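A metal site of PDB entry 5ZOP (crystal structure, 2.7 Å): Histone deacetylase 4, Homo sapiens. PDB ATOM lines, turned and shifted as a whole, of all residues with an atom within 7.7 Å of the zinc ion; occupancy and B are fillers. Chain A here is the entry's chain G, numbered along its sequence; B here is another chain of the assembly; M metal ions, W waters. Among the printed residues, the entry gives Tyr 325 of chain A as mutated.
N of Val 190 is in hydrogen-bond range of OD1 of Asp 283 (2.9 Å). OD2 of Asp 189 sits close to N of Gly 323 (2.9 Å). The backbone NH (N) of Asp 189 lies within hydrogen-bond range of the side-chain carboxylate (OD1) of Asp 187 (3.2 Å). The backbone carbonyl oxygen (O) of Gly 323 sits at hydrogen-bond distance from the backbone NH (N) of Phe 282, at 3.1 Å.
Gly 323 touches the zinc ion. Tyr 325 touches the zinc ion (OH to ZN, 3.8 Å). Within 4 Å of the zinc ion: Asp 189, His 191, Asp 283, Gly 323 and Tyr 325.
The zinc ion is bound by OD2 of Asp 283, ND1 of His 191, OD1 of Asp 189, water W1 and OD2 of Asp 189.
Water W1 lies within hydrogen-bond range of NE2 of His 151, NE2 of His 152 and OH of Tyr 325.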
ATOM      1  N   PRO A 149     -27.654  19.316   2.909  1.00  0.00           N
ATOM      2  CA  PRO A 149     -26.850  19.959   3.958  1.00  0.00           C
ATOM      3  C   PRO A 149     -27.369  21.362   4.243  1.00  0.00           C
ATOM      4  O   PRO A 149     -27.962  22.004   3.370  1.00  0.00           O
ATOM      5  CB  PRO A 149     -25.444  19.995   3.353  1.00  0.00           C
ATOM      6  CG  PRO A 149     -25.670  19.987   1.876  1.00  0.00           C
ATOM      7  CD  PRO A 149     -26.881  19.119   1.670  1.00  0.00           C
ATOM      8  N   HIS A 151     -25.510  23.937   6.363  1.00  0.00           N
ATOM      9  CA  HIS A 151     -24.646  24.914   7.017  1.00  0.00           C
ATOM     10  C   HIS A 151     -24.340  26.139   6.153  1.00  0.00           C
ATOM     11  O   HIS A 151     -23.899  27.157   6.694  1.00  0.00           O
ATOM     12  CB  HIS A 151     -23.349  24.253   7.489  1.00  0.00           C
ATOM     13  CG  HIS A 151     -22.384  23.921   6.399  1.00  0.00           C
ATOM     14  ND1 HIS A 151     -21.024  23.938   6.584  1.00  0.00           N
ATOM     15  CD2 HIS A 151     -22.587  23.550   5.103  1.00  0.00           C
ATOM     16  CE1 HIS A 151     -20.423  23.597   5.453  1.00  0.00           C
ATOM     17  NE2 HIS A 151     -21.349  23.356   4.545  1.00  0.00           N
ATOM     18  N   HIS A 152     -24.559  26.080   4.835  1.00  0.00           N
ATOM     19  CA  HIS A 152     -24.346  27.253   4.002  1.00  0.00           C
ATOM     20  C   HIS A 152     -25.547  28.198   3.939  1.00  0.00           C
ATOM     21  O   HIS A 152     -25.400  29.347   3.513  1.00  0.00           O
ATOM     22  CB  HIS A 152     -23.970  26.853   2.568  1.00  0.00           C
ATOM     23  CG  HIS A 152     -22.619  26.237   2.437  1.00  0.00           C
ATOM     24  ND1 HIS A 152     -21.455  26.913   2.747  1.00  0.00           N
ATOM     25  CD2 HIS A 152     -22.238  25.012   2.015  1.00  0.00           C
ATOM     26  CE1 HIS A 152     -20.420  26.125   2.526  1.00  0.00           C
ATOM     27  NE2 HIS A 152     -20.864  24.969   2.082  1.00  0.00           N
ATOM     28  N   GLY A 160     -25.052  26.794  -1.890  1.00  0.00           N
ATOM     29  CA  GLY A 160     -24.175  25.690  -1.533  1.00  0.00           C
ATOM     30  C   GLY A 160     -24.869  24.372  -1.267  1.00  0.00           C
ATOM     31  O   GLY A 160     -24.457  23.632  -0.368  1.00  0.00           O
ATOM     32  N   PHE A 161     -25.922  24.059  -2.030  1.00  0.00           N
ATOM     33  CA  PHE A 161     -26.798  22.900  -1.822  1.00  0.00           C
ATOM     34  C   PHE A 161     -27.601  22.991  -0.530  1.00  0.00           C
ATOM     35  O   PHE A 161     -28.127  21.975  -0.058  1.00  0.00           O
ATOM     36  CB  PHE A 161     -26.008  21.582  -1.828  1.00  0.00           C
ATOM     37  CG  PHE A 161     -25.020  21.446  -2.949  1.00  0.00           C
ATOM     38  CD1 PHE A 161     -25.363  21.807  -4.247  1.00  0.00           C
ATOM     39  CD2 PHE A 161     -23.751  20.948  -2.706  1.00  0.00           C
ATOM     40  CE1 PHE A 161     -24.441  21.669  -5.279  1.00  0.00           C
ATOM     41  CE2 PHE A 161     -22.836  20.809  -3.731  1.00  0.00           C
ATOM     42  CZ  PHE A 161     -23.186  21.179  -5.020  1.00  0.00           C
ATOM     43  N   CYS A 162     -27.713  24.178   0.056  1.00  0.00           N
ATOM     44  CA  CYS A 162     -28.346  24.354   1.350  1.00  0.00           C
ATOM     45  C   CYS A 162     -29.587  25.238   1.229  1.00  0.00           C
ATOM     46  O   CYS A 162     -29.641  26.156   0.403  1.00  0.00           O
ATOM     47  CB  CYS A 162     -27.384  24.963   2.372  1.00  0.00           C
ATOM     48  SG  CYS A 162     -25.841  24.029   2.577  1.00  0.00           S
ATOM     49  N   ASP A 187     -17.672  22.639  13.227  1.00  0.00           N
ATOM     50  CA  ASP A 187     -17.970  22.530  11.805  1.00  0.00           C
ATOM     51  C   ASP A 187     -16.682  22.098  11.121  1.00  0.00           C
ATOM     52  O   ASP A 187     -15.865  22.942  10.733  1.00  0.00           O
ATOM     53  CB  ASP A 187     -18.496  23.870  11.256  1.00  0.00           C
ATOM     54  CG  ASP A 187     -18.982  23.775   9.818  1.00  0.00           C
ATOM     55  OD1 ASP A 187     -18.536  22.880   9.072  1.00  0.00           O
ATOM     56  OD2 ASP A 187     -19.809  24.624   9.427  1.00  0.00           O
ATOM     57  N   TRP A 188     -16.483  20.787  10.982  1.00  0.00           N
ATOM     58  CA  TRP A 188     -15.298  20.265  10.313  1.00  0.00           C
ATOM     59  C   TRP A 188     -15.569  19.909   8.853  1.00  0.00           C
ATOM     60  O   TRP A 188     -14.764  19.208   8.239  1.00  0.00           O
ATOM     61  CB  TRP A 188     -14.717  19.076  11.081  1.00  0.00           C
ATOM     62  CG  TRP A 188     -15.563  17.835  11.198  1.00  0.00           C
ATOM     63  CD1 TRP A 188     -16.377  17.285  10.248  1.00  0.00           C
ATOM     64  CD2 TRP A 188     -15.652  16.972  12.348  1.00  0.00           C
ATOM     65  NE1 TRP A 188     -16.968  16.142  10.738  1.00  0.00           N
ATOM     66  CE2 TRP A 188     -16.534  15.931  12.018  1.00  0.00           C
ATOM     67  CE3 TRP A 188     -15.062  16.988  13.611  1.00  0.00           C
ATOM     68  CZ2 TRP A 188     -16.851  14.914  12.917  1.00  0.00           C
ATOM     69  CZ3 TRP A 188     -15.372  15.973  14.503  1.00  0.00           C
ATOM     70  CH2 TRP A 188     -16.264  14.951  14.154  1.00  0.00           C
ATOM     71  N   ASP A 189     -16.689  20.361   8.292  1.00  0.00           N
ATOM     72  CA  ASP A 189     -16.848  20.347   6.845  1.00  0.00           C
ATOM     73  C   ASP A 189     -15.778  21.220   6.216  1.00  0.00           C
ATOM     74  O   ASP A 189     -15.403  22.263   6.756  1.00  0.00           O
ATOM     75  CB  ASP A 189     -18.254  20.852   6.469  1.00  0.00           C
ATOM     76  CG  ASP A 189     -18.478  20.895   4.974  1.00  0.00           C
ATOM     77  OD1 ASP A 189     -17.962  21.813   4.304  1.00  0.00           O
ATOM     78  OD2 ASP A 189     -19.171  19.994   4.456  1.00  0.00           O
ATOM     79  N   VAL A 190     -15.254  20.773   5.068  1.00  0.00           N
ATOM     80  CA  VAL A 190     -14.099  21.468   4.500  1.00  0.00           C
ATOM     81  C   VAL A 190     -14.455  22.895   4.074  1.00  0.00           C
ATOM     82  O   VAL A 190     -13.578  23.762   4.024  1.00  0.00           O
ATOM     83  CB  VAL A 190     -13.499  20.656   3.339  1.00  0.00           C
ATOM     84  CG1 VAL A 190     -14.252  20.921   2.040  1.00  0.00           C
ATOM     85  CG2 VAL A 190     -12.008  20.971   3.187  1.00  0.00           C
ATOM     86  N   HIS A 191     -15.721  23.157   3.759  1.00  0.00           N
ATOM     87  CA  HIS A 191     -16.175  24.505   3.475  1.00  0.00           C
ATOM     88  C   HIS A 191     -16.553  25.227   4.766  1.00  0.00           C
ATOM     89  O   HIS A 191     -17.024  24.606   5.722  1.00  0.00           O
ATOM     90  CB  HIS A 191     -17.366  24.495   2.528  1.00  0.00           C
ATOM     91  CG  HIS A 191     -17.149  23.694   1.284  1.00  0.00           C
ATOM     92  ND1 HIS A 191     -17.265  22.318   1.247  1.00  0.00           N
ATOM     93  CD2 HIS A 191     -16.815  24.073   0.024  1.00  0.00           C
ATOM     94  CE1 HIS A 191     -17.018  21.891   0.032  1.00  0.00           C
ATOM     95  NE2 HIS A 191     -16.739  22.935  -0.735  1.00  0.00           N
ATOM     96  N   HIS A 192     -16.354  26.542   4.774  1.00  0.00           N
ATOM     97  CA  HIS A 192     -16.822  27.359   5.892  1.00  0.00           C
ATOM     98  C   HIS A 192     -18.342  27.371   5.946  1.00  0.00           C
ATOM     99  O   HIS A 192     -19.019  27.443   4.914  1.00  0.00           O
ATOM    100  CB  HIS A 192     -16.279  28.785   5.764  1.00  0.00           C
ATOM    101  CG  HIS A 192     -16.736  29.705   6.852  1.00  0.00           C
ATOM    102  ND1 HIS A 192     -17.455  30.856   6.602  1.00  0.00           N
ATOM    103  CD2 HIS A 192     -16.589  29.635   8.194  1.00  0.00           C
ATOM    104  CE1 HIS A 192     -17.723  31.458   7.743  1.00  0.00           C
ATOM    105  NE2 HIS A 192     -17.202  30.741   8.729  1.00  0.00           N
ATOM    106  N   PHE A 219     -11.654  30.376  -1.973  1.00  0.00           N
ATOM    107  CA  PHE A 219     -12.383  29.114  -1.972  1.00  0.00           C
ATOM    108  C   PHE A 219     -13.833  29.403  -1.613  1.00  0.00           C
ATOM    109  O   PHE A 219     -14.157  30.429  -1.009  1.00  0.00           O
ATOM    110  CB  PHE A 219     -11.758  28.125  -0.988  1.00  0.00           C
ATOM    111  CG  PHE A 219     -12.179  26.694  -1.209  1.00  0.00           C
ATOM    112  CD1 PHE A 219     -11.940  26.065  -2.421  1.00  0.00           C
ATOM    113  CD2 PHE A 219     -12.786  25.976  -0.187  1.00  0.00           C
ATOM    114  CE1 PHE A 219     -12.321  24.756  -2.615  1.00  0.00           C
ATOM    115  CE2 PHE A 219     -13.166  24.657  -0.382  1.00  0.00           C
ATOM    116  CZ  PHE A 219     -12.929  24.048  -1.593  1.00  0.00           C
ATOM    117  N   PHE A 220     -14.716  28.485  -1.993  1.00  0.00           N
ATOM    118  CA  PHE A 220     -16.129  28.659  -1.672  1.00  0.00           C
ATOM    119  C   PHE A 220     -16.343  28.516  -0.163  1.00  0.00           C
ATOM    120  O   PHE A 220     -15.776  27.617   0.461  1.00  0.00           O
ATOM    121  CB  PHE A 220     -16.988  27.639  -2.422  1.00  0.00           C
ATOM    122  CG  PHE A 220     -18.462  27.803  -2.184  1.00  0.00           C
ATOM    123  CD1 PHE A 220     -19.213  28.676  -2.961  1.00  0.00           C
ATOM    124  CD2 PHE A 220     -19.113  27.082  -1.187  1.00  0.00           C
ATOM    125  CE1 PHE A 220     -20.574  28.831  -2.745  1.00  0.00           C
ATOM    126  CE2 PHE A 220     -20.466  27.238  -0.965  1.00  0.00           C
ATOM    127  CZ  PHE A 220     -21.197  28.113  -1.750  1.00  0.00           C
ATOM    128  N   GLY A 281     -19.307  17.406   8.077  1.00  0.00           N
ATOM    129  CA  GLY A 281     -18.987  17.301   6.665  1.00  0.00           C
ATOM    130  C   GLY A 281     -17.777  16.397   6.446  1.00  0.00           C
ATOM    131  O   GLY A 281     -16.841  16.375   7.245  1.00  0.00           O
ATOM    132  N   PHE A 282     -17.800  15.657   5.336  1.00  0.00           N
ATOM    133  CA  PHE A 282     -16.753  14.685   5.030  1.00  0.00           C
ATOM    134  C   PHE A 282     -16.038  14.990   3.720  1.00  0.00           C
ATOM    135  O   PHE A 282     -15.356  14.122   3.174  1.00  0.00           O
ATOM    136  CB  PHE A 282     -17.327  13.267   4.998  1.00  0.00           C
ATOM    137  CG  PHE A 282     -17.817  12.779   6.332  1.00  0.00           C
ATOM    138  CD1 PHE A 282     -17.125  13.082   7.486  1.00  0.00           C
ATOM    139  CD2 PHE A 282     -18.973  12.026   6.421  1.00  0.00           C
ATOM    140  CE1 PHE A 282     -17.568  12.636   8.721  1.00  0.00           C
ATOM    141  CE2 PHE A 282     -19.429  11.568   7.656  1.00  0.00           C
ATOM    142  CZ  PHE A 282     -18.724  11.873   8.795  1.00  0.00           C
ATOM    143  N   ASP A 283     -16.181  16.211   3.196  1.00  0.00           N
ATOM    144  CA  ASP A 283     -15.488  16.569   1.968  1.00  0.00           C
ATOM    145  C   ASP A 283     -13.992  16.819   2.174  1.00  0.00           C
ATOM    146  O   ASP A 283     -13.263  16.942   1.185  1.00  0.00           O
ATOM    147  CB  ASP A 283     -16.138  17.804   1.321  1.00  0.00           C
ATOM    148  CG  ASP A 283     -16.824  18.699   2.337  1.00  0.00           C
ATOM    149  OD1 ASP A 283     -16.518  18.592   3.546  1.00  0.00           O
ATOM    150  OD2 ASP A 283     -17.684  19.507   1.925  1.00  0.00           O
ATOM    151  N   ALA A 284     -13.536  16.894   3.421  1.00  0.00           N
ATOM    152  CA  ALA A 284     -12.111  16.970   3.712  1.00  0.00           C
ATOM    153  C   ALA A 284     -11.414  15.619   3.632  1.00  0.00           C
ATOM    154  O   ALA A 284     -10.182  15.572   3.708  1.00  0.00           O
ATOM    155  CB  ALA A 284     -11.889  17.578   5.100  1.00  0.00           C
ATOM    156  N   LEU A 292     -13.891  20.428  -4.901  1.00  0.00           N
ATOM    157  CA  LEU A 292     -14.842  20.148  -3.822  1.00  0.00           C
ATOM    158  C   LEU A 292     -14.169  19.932  -2.465  1.00  0.00           C
ATOM    159  O   LEU A 292     -14.882  19.809  -1.463  1.00  0.00           O
ATOM    160  CB  LEU A 292     -15.686  18.918  -4.160  1.00  0.00           C
ATOM    161  CG  LEU A 292     -16.866  19.180  -5.098  1.00  0.00           C
ATOM    162  CD1 LEU A 292     -17.611  17.897  -5.396  1.00  0.00           C
ATOM    163  CD2 LEU A 292     -17.796  20.222  -4.476  1.00  0.00           C
ATOM    164  N   GLY A 293     -12.845  19.876  -2.417  1.00  0.00           N
ATOM    165  CA  GLY A 293     -12.144  19.689  -1.153  1.00  0.00           C
ATOM    166  C   GLY A 293     -10.641  19.714  -1.324  1.00  0.00           C
ATOM    167  O   GLY A 293     -10.003  20.739  -1.065  1.00  0.00           O
ATOM    168  N   GLU A 322     -23.261  16.982   6.651  1.00  0.00           N
ATOM    169  CA  GLU A 322     -23.270  18.185   5.841  1.00  0.00           C
ATOM    170  C   GLU A 322     -22.765  17.864   4.440  1.00  0.00           C
ATOM    171  O   GLU A 322     -23.490  17.282   3.632  1.00  0.00           O
ATOM    172  CB  GLU A 322     -22.418  19.283   6.475  1.00  0.00           C
ATOM    173  CG  GLU A 322     -22.937  19.789   7.811  1.00  0.00           C
ATOM    174  CD  GLU A 322     -24.134  20.718   7.669  1.00  0.00           C
ATOM    175  OE1 GLU A 322     -24.798  20.991   8.693  1.00  0.00           O
ATOM    176  OE2 GLU A 322     -24.403  21.165   6.543  1.00  0.00           O
ATOM    177  N   GLY A 323     -21.505  18.217   4.156  1.00  0.00           N
ATOM    178  CA  GLY A 323     -20.898  17.937   2.879  1.00  0.00           C
ATOM    179  C   GLY A 323     -20.260  16.557   2.836  1.00  0.00           C
ATOM    180  O   GLY A 323     -20.466  15.714   3.711  1.00  0.00           O
ATOM    181  N   GLY A 324     -19.467  16.338   1.799  1.00  0.00           N
ATOM    182  CA  GLY A 324     -18.899  15.038   1.532  1.00  0.00           C
ATOM    183  C   GLY A 324     -19.627  14.368   0.385  1.00  0.00           C
ATOM    184  O   GLY A 324     -20.825  14.073   0.491  1.00  0.00           O
ATOM    185  N   TYR A 325     -18.922  14.135  -0.718  1.00  0.00           N
ATOM    186  CA  TYR A 325     -19.568  13.742  -1.966  1.00  0.00           C
ATOM    187  C   TYR A 325     -18.984  12.490  -2.615  1.00  0.00           C
ATOM    188  O   TYR A 325     -19.649  11.918  -3.490  1.00  0.00           O
ATOM    189  CB  TYR A 325     -19.527  14.901  -2.967  1.00  0.00           C
ATOM    190  CG  TYR A 325     -19.924  16.210  -2.319  1.00  0.00           C
ATOM    191  CD1 TYR A 325     -21.265  16.564  -2.176  1.00  0.00           C
ATOM    192  CD2 TYR A 325     -18.962  17.097  -1.833  1.00  0.00           C
ATOM    193  CE1 TYR A 325     -21.626  17.748  -1.581  1.00  0.00           C
ATOM    194  CE2 TYR A 325     -19.323  18.282  -1.238  1.00  0.00           C
ATOM    195  CZ  TYR A 325     -20.661  18.607  -1.112  1.00  0.00           C
ATOM    196  OH  TYR A 325     -21.022  19.791  -0.516  1.00  0.00           O
ATOM    197  N   ILE B   4     -19.920  26.409  -5.574  1.00  0.00           N
ATOM    198  CA  ILE B   4     -19.347  25.346  -4.755  1.00  0.00           C
ATOM    199  C   ILE B   4     -18.869  24.181  -5.619  1.00  0.00           C
ATOM    200  O   ILE B   4     -17.947  23.460  -5.219  1.00  0.00           O
ATOM    201  CB  ILE B   4     -20.369  24.900  -3.697  1.00  0.00           C
ATOM    202  CG1 ILE B   4     -19.718  23.933  -2.699  1.00  0.00           C
ATOM    203  CG2 ILE B   4     -21.592  24.263  -4.349  1.00  0.00           C
ATOM    204  CD1 ILE B   4     -20.638  23.511  -1.560  1.00  0.00           C
HETATM  205 ZN    ZN M   1     -18.799  21.225   2.268  1.00  0.00          ZN
HETATM  206  O   HOH W   1     -21.031  21.874   2.094  1.00  0.00           O
